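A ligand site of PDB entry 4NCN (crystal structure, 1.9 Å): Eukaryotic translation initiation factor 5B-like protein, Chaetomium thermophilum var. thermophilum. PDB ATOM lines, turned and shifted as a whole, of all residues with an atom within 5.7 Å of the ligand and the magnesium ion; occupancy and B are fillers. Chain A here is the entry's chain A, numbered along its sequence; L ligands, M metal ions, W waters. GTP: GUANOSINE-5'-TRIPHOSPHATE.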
ATOM      1  N   GLY A  17      14.457 -21.221  20.078  1.00  0.00           N
ATOM      2  CA  GLY A  17      14.480 -20.704  21.431  1.00  0.00           C
ATOM      3  C   GLY A  17      13.762 -19.368  21.523  1.00  0.00           C
ATOM      4  O   GLY A  17      13.503 -18.690  20.503  1.00  0.00           O
ATOM      5  N   HIS A  18      13.558 -18.939  22.772  1.00  0.00           N
ATOM      6  CA  HIS A  18      12.852 -17.702  23.041  1.00  0.00           C
ATOM      7  C   HIS A  18      13.624 -16.493  22.445  1.00  0.00           C
ATOM      8  O   HIS A  18      14.815 -16.552  22.137  1.00  0.00           O
ATOM      9  CB  HIS A  18      12.628 -17.577  24.564  1.00  0.00           C
ATOM     10  CG  HIS A  18      11.682 -16.480  24.967  1.00  0.00           C
ATOM     11  ND1 HIS A  18      10.303 -16.609  24.905  1.00  0.00           N
ATOM     12  CD2 HIS A  18      11.928 -15.249  25.457  1.00  0.00           C
ATOM     13  CE1 HIS A  18       9.742 -15.490  25.342  1.00  0.00           C
ATOM     14  NE2 HIS A  18      10.710 -14.647  25.682  1.00  0.00           N
ATOM     15  N   VAL A  19      12.920 -15.390  22.293  1.00  0.00           N
ATOM     16  CA  VAL A  19      13.536 -14.217  21.660  1.00  0.00           C
ATOM     17  C   VAL A  19      14.768 -13.713  22.460  1.00  0.00           C
ATOM     18  O   VAL A  19      14.798 -13.752  23.724  1.00  0.00           O
ATOM     19  CB  VAL A  19      12.517 -13.040  21.468  1.00  0.00           C
ATOM     20  CG1 VAL A  19      12.150 -12.372  22.858  1.00  0.00           C
ATOM     21  CG2 VAL A  19      13.106 -11.975  20.503  1.00  0.00           C
ATOM     22  N   ASP A  20      15.804 -13.326  21.703  1.00  0.00           N
ATOM     23  CA  ASP A  20      17.039 -12.755  22.234  1.00  0.00           C
ATOM     24  C   ASP A  20      17.857 -13.693  23.142  1.00  0.00           C
ATOM     25  O   ASP A  20      18.678 -13.215  23.923  1.00  0.00           O
ATOM     26  CB  ASP A  20      16.746 -11.428  23.009  1.00  0.00           C
ATOM     27  CG  ASP A  20      16.485 -10.271  22.038  1.00  0.00           C
ATOM     28  OD1 ASP A  20      15.850  -9.282  22.447  1.00  0.00           O
ATOM     29  OD2 ASP A  20      16.864 -10.424  20.835  1.00  0.00           O
ATOM     30  N   THR A  21      17.663 -15.010  23.027  1.00  0.00           N
ATOM     31  CA  THR A  21      18.443 -15.933  23.870  1.00  0.00           C
ATOM     32  C   THR A  21      19.836 -16.134  23.324  1.00  0.00           C
ATOM     33  O   THR A  21      20.669 -16.620  24.058  1.00  0.00           O
ATOM     34  CB  THR A  21      17.731 -17.283  24.034  1.00  0.00           C
ATOM     35  OG1 THR A  21      17.306 -17.723  22.721  1.00  0.00           O
ATOM     36  CG2 THR A  21      16.476 -17.025  24.940  1.00  0.00           C
ATOM     37  N   GLY A  22      20.068 -15.763  22.054  1.00  0.00           N
ATOM     38  CA  GLY A  22      21.430 -15.752  21.475  1.00  0.00           C
ATOM     39  C   GLY A  22      21.645 -16.818  20.379  1.00  0.00           C
ATOM     40  O   GLY A  22      22.762 -17.196  20.067  1.00  0.00           O
ATOM     41  N   LYS A  23      20.567 -17.302  19.779  1.00  0.00           N
ATOM     42  CA  LYS A  23      20.700 -18.243  18.665  1.00  0.00           C
ATOM     43  C   LYS A  23      21.624 -17.721  17.555  1.00  0.00           C
ATOM     44  O   LYS A  23      22.608 -18.385  17.078  1.00  0.00           O
ATOM     45  CB  LYS A  23      19.303 -18.505  18.043  1.00  0.00           C
ATOM     46  CG  LYS A  23      18.195 -19.043  19.041  1.00  0.00           C
ATOM     47  CD  LYS A  23      16.799 -19.173  18.396  1.00  0.00           C
ATOM     48  CE  LYS A  23      16.160 -17.824  18.112  1.00  0.00           C
ATOM     49  NZ  LYS A  23      15.707 -17.012  19.412  1.00  0.00           N
ATOM     50  N   THR A  24      21.278 -16.533  17.093  1.00  0.00           N
ATOM     51  CA  THR A  24      22.017 -15.966  15.967  1.00  0.00           C
ATOM     52  C   THR A  24      23.425 -15.564  16.455  1.00  0.00           C
ATOM     53  O   THR A  24      24.376 -15.762  15.722  1.00  0.00           O
ATOM     54  CB  THR A  24      21.278 -14.728  15.346  1.00  0.00           C
ATOM     55  OG1 THR A  24      19.998 -15.158  14.852  1.00  0.00           O
ATOM     56  CG2 THR A  24      22.076 -14.155  14.129  1.00  0.00           C
ATOM     57  N   LYS A  25      23.546 -14.969  17.649  1.00  0.00           N
ATOM     58  CA  LYS A  25      24.856 -14.625  18.169  1.00  0.00           C
ATOM     59  C   LYS A  25      25.768 -15.889  18.252  1.00  0.00           C
ATOM     60  O   LYS A  25      27.007 -15.801  17.928  1.00  0.00           O
ATOM     61  CB  LYS A  25      24.729 -13.889  19.544  1.00  0.00           C
ATOM     62  CG  LYS A  25      25.901 -12.965  19.852  1.00  0.00           C
ATOM     63  CD  LYS A  25      25.859 -11.723  18.912  1.00  0.00           C
ATOM     64  CE  LYS A  25      27.073 -10.801  19.150  1.00  0.00           C
ATOM     65  NZ  LYS A  25      26.886  -9.580  18.310  1.00  0.00           N
ATOM     66  N   LEU A  26      25.209 -17.048  18.634  1.00  0.00           N
ATOM     67  CA  LEU A  26      26.034 -18.284  18.654  1.00  0.00           C
ATOM     68  C   LEU A  26      26.521 -18.648  17.254  1.00  0.00           C
ATOM     69  O   LEU A  26      27.719 -18.958  17.032  1.00  0.00           O
ATOM     70  CB  LEU A  26      25.218 -19.468  19.231  1.00  0.00           C
ATOM     71  CG  LEU A  26      25.016 -19.418  20.710  1.00  0.00           C
ATOM     72  CD1 LEU A  26      23.834 -20.420  21.137  1.00  0.00           C
ATOM     73  CD2 LEU A  26      26.348 -19.787  21.500  1.00  0.00           C
ATOM     74  N   GLN A  36      23.931 -10.656  13.396  1.00  0.00           N
ATOM     75  CA  GLN A  36      23.021 -10.111  14.426  1.00  0.00           C
ATOM     76  C   GLN A  36      23.115  -8.621  14.476  1.00  0.00           C
ATOM     77  O   GLN A  36      22.082  -7.914  14.680  1.00  0.00           O
ATOM     78  CB  GLN A  36      23.349 -10.698  15.818  1.00  0.00           C
ATOM     79  CG  GLN A  36      22.251 -10.529  16.865  1.00  0.00           C
ATOM     80  CD  GLN A  36      22.242  -9.210  17.569  1.00  0.00           C
ATOM     81  OE1 GLN A  36      23.259  -8.541  17.647  1.00  0.00           O
ATOM     82  NE2 GLN A  36      21.072  -8.843  18.175  1.00  0.00           N
ATOM     83  N   GLU A  39      20.832  -6.892  11.970  1.00  0.00           N
ATOM     84  CA  GLU A  39      19.385  -7.148  11.953  1.00  0.00           C
ATOM     85  C   GLU A  39      18.583  -5.950  12.452  1.00  0.00           C
ATOM     86  O   GLU A  39      18.929  -5.348  13.457  1.00  0.00           O
ATOM     87  CB  GLU A  39      19.058  -8.366  12.812  1.00  0.00           C
ATOM     88  CG  GLU A  39      19.464  -9.738  12.146  1.00  0.00           C
ATOM     89  CD  GLU A  39      19.197 -10.913  13.069  1.00  0.00           C
ATOM     90  OE1 GLU A  39      19.251 -10.729  14.330  1.00  0.00           O
ATOM     91  OE2 GLU A  39      18.932 -12.050  12.555  1.00  0.00           O
ATOM     92  N   GLY A  42      17.577  -5.938  16.132  1.00  0.00           N
ATOM     93  CA  GLY A  42      18.384  -7.005  16.733  1.00  0.00           C
ATOM     94  C   GLY A  42      17.615  -8.304  16.752  1.00  0.00           C
ATOM     95  O   GLY A  42      17.917  -9.179  17.563  1.00  0.00           O
ATOM     96  N   ILE A  43      16.610  -8.482  15.857  1.00  0.00           N
ATOM     97  CA  ILE A  43      15.870  -9.741  15.895  1.00  0.00           C
ATOM     98  C   ILE A  43      15.851 -10.406  14.525  1.00  0.00           C
ATOM     99  O   ILE A  43      15.848  -9.765  13.479  1.00  0.00           O
ATOM    100  CB  ILE A  43      14.398  -9.576  16.373  1.00  0.00           C
ATOM    101  CG1 ILE A  43      13.686  -8.550  15.544  1.00  0.00           C
ATOM    102  CG2 ILE A  43      14.291  -9.115  17.846  1.00  0.00           C
ATOM    103  CD1 ILE A  43      12.114  -8.660  15.717  1.00  0.00           C
ATOM    104  N   THR A  44      15.855 -11.714  14.550  1.00  0.00           N
ATOM    105  CA  THR A  44      15.708 -12.531  13.328  1.00  0.00           C
ATOM    106  C   THR A  44      14.223 -12.525  12.890  1.00  0.00           C
ATOM    107  O   THR A  44      13.338 -12.700  13.709  1.00  0.00           O
ATOM    108  CB  THR A  44      16.217 -13.920  13.623  1.00  0.00           C
ATOM    109  OG1 THR A  44      17.598 -13.829  14.034  1.00  0.00           O
ATOM    110  CG2 THR A  44      16.125 -14.862  12.388  1.00  0.00           C
ATOM    111  N   ASP A  81      18.612 -21.291  11.177  1.00  0.00           N
ATOM    112  CA  ASP A  81      18.399 -20.292  12.225  1.00  0.00           C
ATOM    113  C   ASP A  81      16.924 -19.914  12.144  1.00  0.00           C
ATOM    114  O   ASP A  81      16.356 -19.867  11.031  1.00  0.00           O
ATOM    115  CB  ASP A  81      19.315 -19.060  11.974  1.00  0.00           C
ATOM    116  CG  ASP A  81      19.387 -18.124  13.200  1.00  0.00           C
ATOM    117  OD1 ASP A  81      18.810 -18.496  14.240  1.00  0.00           O
ATOM    118  OD2 ASP A  81      20.001 -17.046  13.123  1.00  0.00           O
ATOM    119  N   THR A  82      16.285 -19.700  13.283  1.00  0.00           N
ATOM    120  CA  THR A  82      14.870 -19.291  13.262  1.00  0.00           C
ATOM    121  C   THR A  82      14.601 -18.115  14.188  1.00  0.00           C
ATOM    122  O   THR A  82      15.373 -17.917  15.122  1.00  0.00           O
ATOM    123  CB  THR A  82      13.908 -20.429  13.723  1.00  0.00           C
ATOM    124  OG1 THR A  82      14.196 -20.761  15.088  1.00  0.00           O
ATOM    125  CG2 THR A  82      14.015 -21.677  12.810  1.00  0.00           C
ATOM    126  N   PRO A  83      13.515 -17.343  13.933  1.00  0.00           N
ATOM    127  CA  PRO A  83      13.171 -16.274  14.885  1.00  0.00           C
ATOM    128  C   PRO A  83      12.688 -16.787  16.185  1.00  0.00           C
ATOM    129  O   PRO A  83      12.007 -17.831  16.207  1.00  0.00           O
ATOM    130  CB  PRO A  83      11.996 -15.519  14.218  1.00  0.00           C
ATOM    131  CG  PRO A  83      12.099 -15.897  12.683  1.00  0.00           C
ATOM    132  CD  PRO A  83      12.720 -17.316  12.682  1.00  0.00           C
ATOM    133  N   GLY A  84      12.950 -16.033  17.263  1.00  0.00           N
ATOM    134  CA  GLY A  84      12.330 -16.372  18.544  1.00  0.00           C
ATOM    135  C   GLY A  84      11.177 -15.414  18.823  1.00  0.00           C
ATOM    136  O   GLY A  84      10.392 -15.672  19.727  1.00  0.00           O
ATOM    137  N   HIS A  85      11.068 -14.310  18.105  1.00  0.00           N
ATOM    138  CA  HIS A  85       9.985 -13.353  18.376  1.00  0.00           C
ATOM    139  C   HIS A  85       8.605 -14.065  18.296  1.00  0.00           C
ATOM    140  O   HIS A  85       8.415 -14.917  17.434  1.00  0.00           O
ATOM    141  CB  HIS A  85       9.997 -12.173  17.404  1.00  0.00           C
ATOM    142  CG  HIS A  85       9.014 -11.091  17.752  1.00  0.00           C
ATOM    143  ND1 HIS A  85       7.699 -11.134  17.364  1.00  0.00           N
ATOM    144  CD2 HIS A  85       9.171  -9.946  18.454  1.00  0.00           C
ATOM    145  CE1 HIS A  85       7.065 -10.069  17.818  1.00  0.00           C
ATOM    146  NE2 HIS A  85       7.931  -9.329  18.513  1.00  0.00           N
ATOM    147  N   ASN A 135      22.882 -20.717  27.435  1.00  0.00           N
ATOM    148  CA  ASN A 135      23.707 -19.595  26.950  1.00  0.00           C
ATOM    149  C   ASN A 135      23.773 -18.373  27.914  1.00  0.00           C
ATOM    150  O   ASN A 135      23.000 -18.267  28.860  1.00  0.00           O
ATOM    151  CB  ASN A 135      23.133 -19.168  25.577  1.00  0.00           C
ATOM    152  CG  ASN A 135      24.069 -18.256  24.842  1.00  0.00           C
ATOM    153  OD1 ASN A 135      25.289 -18.488  24.871  1.00  0.00           O
ATOM    154  ND2 ASN A 135      23.535 -17.192  24.202  1.00  0.00           N
ATOM    155  N   LYS A 136      24.771 -17.501  27.681  1.00  0.00           N
ATOM    156  CA  LYS A 136      25.060 -16.295  28.455  1.00  0.00           C
ATOM    157  C   LYS A 136      25.750 -16.639  29.762  1.00  0.00           C
ATOM    158  O   LYS A 136      25.616 -15.907  30.703  1.00  0.00           O
ATOM    159  CB  LYS A 136      23.804 -15.434  28.666  1.00  0.00           C
ATOM    160  CG  LYS A 136      23.043 -15.187  27.268  1.00  0.00           C
ATOM    161  CD  LYS A 136      22.117 -13.951  27.278  1.00  0.00           C
ATOM    162  CE  LYS A 136      21.448 -13.748  25.819  1.00  0.00           C
ATOM    163  NZ  LYS A 136      20.538 -12.538  25.985  1.00  0.00           N
ATOM    164  N   ILE A 137      26.591 -17.688  29.799  1.00  0.00           N
ATOM    165  CA  ILE A 137      27.269 -17.925  31.093  1.00  0.00           C
ATOM    166  C   ILE A 137      28.250 -16.831  31.515  1.00  0.00           C
ATOM    167  O   ILE A 137      28.615 -16.768  32.665  1.00  0.00           O
ATOM    168  CB  ILE A 137      28.008 -19.234  31.093  1.00  0.00           C
ATOM    169  CG1 ILE A 137      29.100 -19.221  30.025  1.00  0.00           C
ATOM    170  CG2 ILE A 137      27.002 -20.392  30.952  1.00  0.00           C
ATOM    171  CD1 ILE A 137      29.808 -20.624  29.932  1.00  0.00           C
ATOM    172  N   ASP A 138      28.661 -15.985  30.587  1.00  0.00           N
ATOM    173  CA  ASP A 138      29.528 -14.869  30.931  1.00  0.00           C
ATOM    174  C   ASP A 138      28.796 -13.838  31.832  1.00  0.00           C
ATOM    175  O   ASP A 138      29.445 -12.962  32.438  1.00  0.00           O
ATOM    176  CB  ASP A 138      30.021 -14.210  29.631  1.00  0.00           C
ATOM    177  CG  ASP A 138      28.856 -13.661  28.810  1.00  0.00           C
ATOM    178  OD1 ASP A 138      28.548 -12.439  28.978  1.00  0.00           O
ATOM    179  OD2 ASP A 138      28.161 -14.457  28.115  1.00  0.00           O
ATOM    180  N   ARG A 139      27.465 -13.913  31.932  1.00  0.00           N
ATOM    181  CA  ARG A 139      26.697 -13.012  32.818  1.00  0.00           C
ATOM    182  C   ARG A 139      26.707 -13.485  34.266  1.00  0.00           C
ATOM    183  O   ARG A 139      26.186 -12.801  35.136  1.00  0.00           O
ATOM    184  CB  ARG A 139      25.262 -12.869  32.343  1.00  0.00           C
ATOM    185  CG  ARG A 139      25.182 -12.381  30.908  1.00  0.00           C
ATOM    186  CD  ARG A 139      25.233 -10.905  30.814  1.00  0.00           C
ATOM    187  NE  ARG A 139      24.120 -10.303  31.542  1.00  0.00           N
ATOM    188  CZ  ARG A 139      23.824  -9.013  31.544  1.00  0.00           C
ATOM    189  NH1 ARG A 139      24.530  -8.163  30.795  1.00  0.00           N
ATOM    190  NH2 ARG A 139      22.816  -8.581  32.267  1.00  0.00           N
ATOM    191  N   THR A 202      27.053 -22.321  27.467  1.00  0.00           N
ATOM    192  CA  THR A 202      27.749 -21.600  26.412  1.00  0.00           C
ATOM    193  C   THR A 202      27.803 -20.125  26.642  1.00  0.00           C
ATOM    194  O   THR A 202      27.000 -19.574  27.404  1.00  0.00           O
ATOM    195  CB  THR A 202      27.081 -21.801  25.032  1.00  0.00           C
ATOM    196  OG1 THR A 202      25.721 -21.288  25.044  1.00  0.00           O
ATOM    197  CG2 THR A 202      27.049 -23.273  24.661  1.00  0.00           C
ATOM    198  N   SER A 203      28.738 -19.476  25.952  1.00  0.00           N
ATOM    199  CA  SER A 203      28.655 -18.038  25.809  1.00  0.00           C
ATOM    200  C   SER A 203      28.879 -17.703  24.379  1.00  0.00           C
ATOM    201  O   SER A 203      29.972 -17.979  23.824  1.00  0.00           O
ATOM    202  CB  SER A 203      29.687 -17.325  26.663  1.00  0.00           C
ATOM    203  OG  SER A 203      29.649 -15.945  26.368  1.00  0.00           O
ATOM    204  N   ALA A 204      27.888 -17.074  23.729  1.00  0.00           N
ATOM    205  CA  ALA A 204      28.139 -16.568  22.348  1.00  0.00           C
ATOM    206  C   ALA A 204      29.105 -15.402  22.346  1.00  0.00           C
ATOM    207  O   ALA A 204      29.788 -15.109  21.350  1.00  0.00           O
ATOM    208  CB  ALA A 204      26.739 -16.114  21.662  1.00  0.00           C
ATOM    209  N   HIS A 205      29.214 -14.690  23.463  1.00  0.00           N
ATOM    210  CA  HIS A 205      30.167 -13.554  23.488  1.00  0.00           C
ATOM    211  C   HIS A 205      31.619 -14.007  23.649  1.00  0.00           C
ATOM    212  O   HIS A 205      32.532 -13.513  22.957  1.00  0.00           O
ATOM    213  CB  HIS A 205      29.780 -12.568  24.624  1.00  0.00           C
ATOM    214  CG  HIS A 205      28.645 -11.651  24.233  1.00  0.00           C
ATOM    215  ND1 HIS A 205      28.274 -10.534  24.950  1.00  0.00           N
ATOM    216  CD2 HIS A 205      27.820 -11.694  23.152  1.00  0.00           C
ATOM    217  CE1 HIS A 205      27.248  -9.937  24.355  1.00  0.00           C
ATOM    218  NE2 HIS A 205      26.944 -10.629  23.262  1.00  0.00           N
ATOM    219  N   THR A 206      31.874 -14.932  24.576  1.00  0.00           N
ATOM    220  CA  THR A 206      33.292 -15.394  24.763  1.00  0.00           C
ATOM    221  C   THR A 206      33.634 -16.614  23.931  1.00  0.00           C
ATOM    222  O   THR A 206      34.857 -16.905  23.698  1.00  0.00           O
ATOM    223  CB  THR A 206      33.621 -15.787  26.227  1.00  0.00           C
ATOM    224  OG1 THR A 206      32.900 -17.008  26.558  1.00  0.00           O
ATOM    225  CG2 THR A 206      33.192 -14.665  27.182  1.00  0.00           C
ATOM    226  N   ARG A 293      20.329 -16.302   4.146  1.00  0.00           N
ATOM    227  CA  ARG A 293      19.404 -15.152   4.204  1.00  0.00           C
ATOM    228  C   ARG A 293      20.167 -13.817   3.973  1.00  0.00           C
ATOM    229  O   ARG A 293      19.610 -12.740   4.134  1.00  0.00           O
ATOM    230  CB  ARG A 293      18.600 -15.120   5.517  1.00  0.00           C
ATOM    231  CG  ARG A 293      19.387 -14.890   6.816  1.00  0.00           C
ATOM    232  CD  ARG A 293      18.435 -14.893   7.985  1.00  0.00           C
ATOM    233  NE  ARG A 293      19.089 -15.145   9.273  1.00  0.00           N
ATOM    234  CZ  ARG A 293      19.255 -14.213  10.216  1.00  0.00           C
ATOM    235  NH1 ARG A 293      18.831 -12.951   9.998  1.00  0.00           N
ATOM    236  NH2 ARG A 293      19.811 -14.562  11.381  1.00  0.00           N
HETATM  237  PG  GTP L   1      15.882 -13.709  17.974  1.00  0.00           P
HETATM  238  O1G GTP L   1      16.361 -14.263  16.676  1.00  0.00           O
HETATM  239  O2G GTP L   1      14.883 -14.637  18.624  1.00  0.00           O
HETATM  240  O3G GTP L   1      15.511 -12.261  17.841  1.00  0.00           O
HETATM  241  O3B GTP L   1      17.192 -13.522  18.954  1.00  0.00           O
HETATM  242  PB  GTP L   1      18.424 -14.558  19.132  1.00  0.00           P
HETATM  243  O1B GTP L   1      18.088 -15.748  19.992  1.00  0.00           O
HETATM  244  O2B GTP L   1      19.051 -14.952  17.791  1.00  0.00           O
HETATM  245  O3A GTP L   1      19.488 -13.751  19.996  1.00  0.00           O
HETATM  246  PA  GTP L   1      20.511 -12.615  19.423  1.00  0.00           P
HETATM  247  O1A GTP L   1      21.683 -13.235  18.747  1.00  0.00           O
HETATM  248  O2A GTP L   1      19.739 -11.612  18.585  1.00  0.00           O
HETATM  249  O5' GTP L   1      21.056 -11.975  20.786  1.00  0.00           O
HETATM  250  C5' GTP L   1      20.210 -11.139  21.596  1.00  0.00           C
HETATM  251  C4' GTP L   1      21.111 -10.231  22.460  1.00  0.00           C
HETATM  252  O4' GTP L   1      21.746 -11.125  23.382  1.00  0.00           O
HETATM  253  C3' GTP L   1      22.243  -9.541  21.692  1.00  0.00           C
HETATM  254  O3' GTP L   1      22.424  -8.280  22.271  1.00  0.00           O
HETATM  255  C2' GTP L   1      23.438 -10.362  22.041  1.00  0.00           C
HETATM  256  O2' GTP L   1      24.683  -9.691  21.893  1.00  0.00           O
HETATM  257  C1' GTP L   1      23.106 -10.862  23.462  1.00  0.00           C
HETATM  258  N9  GTP L   1      23.776 -12.183  23.647  1.00  0.00           N
HETATM  259  C8  GTP L   1      23.640 -13.334  22.867  1.00  0.00           C
HETATM  260  N7  GTP L   1      24.474 -14.278  23.426  1.00  0.00           N
HETATM  261  C5  GTP L   1      25.054 -13.748  24.526  1.00  0.00           C
HETATM  262  C6  GTP L   1      25.950 -14.237  25.474  1.00  0.00           C
HETATM  263  O6  GTP L   1      26.399 -15.380  25.372  1.00  0.00           O
HETATM  264  N1  GTP L   1      26.419 -13.404  26.466  1.00  0.00           N
HETATM  265  C2  GTP L   1      25.946 -12.108  26.597  1.00  0.00           C
HETATM  266  N2  GTP L   1      26.337 -11.273  27.592  1.00  0.00           N
HETATM  267  N3  GTP L   1      25.048 -11.665  25.709  1.00  0.00           N
HETATM  268  C4  GTP L   1      24.621 -12.453  24.671  1.00  0.00           C
HETATM  269 MG    MG M   1      18.273 -14.461  15.956  1.00  0.00          MG
HETATM  270  O   HOH W   1      25.592  -8.543  27.820  1.00  0.00           O
HETATM  271  O   HOH W   2      13.043 -13.151  16.531  1.00  0.00           O
HETATM  272  O   HOH W   3      17.728 -16.525  15.468  1.00  0.00           O
HETATM  273  O   HOH W   4      25.473  -6.620  22.191  1.00  0.00           O
HETATM  274  O   HOH W   5      18.911 -12.470  16.279  1.00  0.00           O
HETATM  275  O   HOH W   6      22.395 -10.331  26.788  1.00  0.00           O
HETATM  276  O   HOH W   7      20.334  -6.802  20.072  1.00  0.00           O
HETATM  277  O   HOH W   8      24.987  -8.084  19.652  1.00  0.00           O
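N of Thr 44 sits at hydrogen-bond distance from O3G of the ligand, 3.4 Å away.
The backbone NH (N) of Thr 24 lies close to an oxygen (O2B) of the ligand, 2.8 Å away.
The side-chain carboxylate (OD2) of Asp 138 sits at hydrogen-bond distance from a nitrogen (N1) of the ligand (2.6 Å).
An oxygen (O1B) of the ligand is in hydrogen-bond range of the backbone NH of Lys 23 (2.9 Å).
The side-chain amino group of Lys 23 lies within salt-bridge range of an oxygen (O2G) of the ligand (2.6 Å).
N of Gly 84 sits at hydrogen-bond distance from O2G of the ligand, at 2.7 Å.
O1A of the ligand sits at hydrogen-bond distance from N of Lys 25 (2.8 Å).
N of Ala 204 lies within hydrogen-bond range of O6 of the ligand, 2.8 Å away.
N of His 205 sits at hydrogen-bond distance from O6 of the ligand (3.5 Å).
NE2 of His 205 sits at hydrogen-bond distance from O2' of the ligand (2.8 Å).
The backbone NH of Gly 22 lies within hydrogen-bond range of an oxygen (O1B) of the ligand (2.9 Å).
The backbone NH (N) of Asp 20 sits at hydrogen-bond distance from an oxygen (O3B) of the ligand (3.1 Å).
NE2 of Gln 36 sits at hydrogen-bond distance from O2A of the ligand, 3.1 Å away.
O1B of the ligand is in hydrogen-bond range of N of Thr 21 (3.2 Å).
O1B of the ligand sits at hydrogen-bond distance from OG1 of Thr 21, 3.5 Å away.
A nitrogen (N7) of the ligand lies within hydrogen-bond range of the side-chain amide nitrogen of Asn 135 (3.2 Å).
NZ of Lys 136 is in hydrogen-bond range of O4' of the ligand (3.2 Å).
The side-chain hydroxyl (OG) of Ser 203 is in hydrogen-bond range of an oxygen (O6) of the ligand.
OG1 of Thr 44 lies close to OE2 of Glu 39 (2.7 Å).
NZ of Lys 23 is in hydrogen-bond range of O of His 18 (2.9 Å).
NZ of Lys 23 is in hydrogen-bond range of O of Gly 17, 3.0 Å away.
The backbone NH of Ala 204 is in hydrogen-bond range of the side-chain amide oxygen of Asn 135.
The backbone carbonyl oxygen of Asp 20 lies within hydrogen-bond range of the side-chain amino group of Lys 136.
The side-chain amide nitrogen of Asn 135 is in hydrogen-bond range of the backbone carbonyl oxygen of Thr 21 (2.9 Å).
OD1 of Asn 135 is in hydrogen-bond range of OG1 of Thr 202, at 2.8 Å.
The backbone NH (N) of Lys 136 lies within hydrogen-bond range of the backbone carbonyl oxygen (O) of Thr 202, at 3.1 Å.
The backbone carbonyl oxygen (O) of Gly 42 sits close to an oxygen (O2A) of the ligand (3.2 Å).
His 18 touches the ligand.
Val 19 touches the ligand (CA to O2G, 3.3 Å).
Ile 43 touches the ligand.
Pro 83 touches the ligand (C to O2G, 3.9 Å).
N of His 85 touches O2G of the ligand, at 3.9 Å.
Arg 139 touches the ligand (CD to N2, 3.4 Å).
Within 4 Å of the ligand: His 18, Val 19, Asp 20, Thr 21, Gly 22, Lys 23, Thr 24, Lys 25, Gln 36, Gly 42, Ile 43, Thr 44, Pro 83, Gly 84, His 85, Asn 135, Lys 136, Asp 138, Arg 139, Ser 203, Ala 204 and His 205.
The nearest printed residue that does not touch the ligand is Thr 82 (4.1 Å).
Two residues have an atom within 4 Å of the magnesium ion: Thr 24 and Thr 44.
Along chain A the residues within 4 Å of the magnesium ion span positions 24 to 44.
The nearest printed residue that does not touch the magnesium ion is Glu 39 (4.2 Å).
The magnesium ion is bound by an oxygen (O1G) of the ligand (2.1 Å), an oxygen (O2B) of the ligand (2.1 Å), water W5 (2.1 Å), the side-chain hydroxyl of Thr 44 (2.1 Å), the side-chain hydroxyl of Thr 24 (2.2 Å) and water W3 (2.2 Å).
Water W5 lies within hydrogen-bond range of an oxygen (O2A) of the ligand and the side-chain carboxylate of Glu 39.
Water W3 lies within hydrogen-bond range of OD1 of Asp 81 (2.6 Å) and O of Thr 82 (2.8 Å).
Water W8 lies within hydrogen-bond range of the side-chain amide oxygen of Gln 36, the side-chain amino group of Lys 25 and an oxygen (O2') of the ligand.
Water W1 lies within hydrogen-bond range of N2 of the ligand (2.8 Å) and NH1 of Arg 139 (3.2 Å).
Water W6 lies within hydrogen-bond range of NZ of Lys 136 and N3 of the ligand.
Water W7 lies within hydrogen-bond range of NE2 of Gln 36 (2.9 Å) and O3' of the ligand (3.4 Å).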
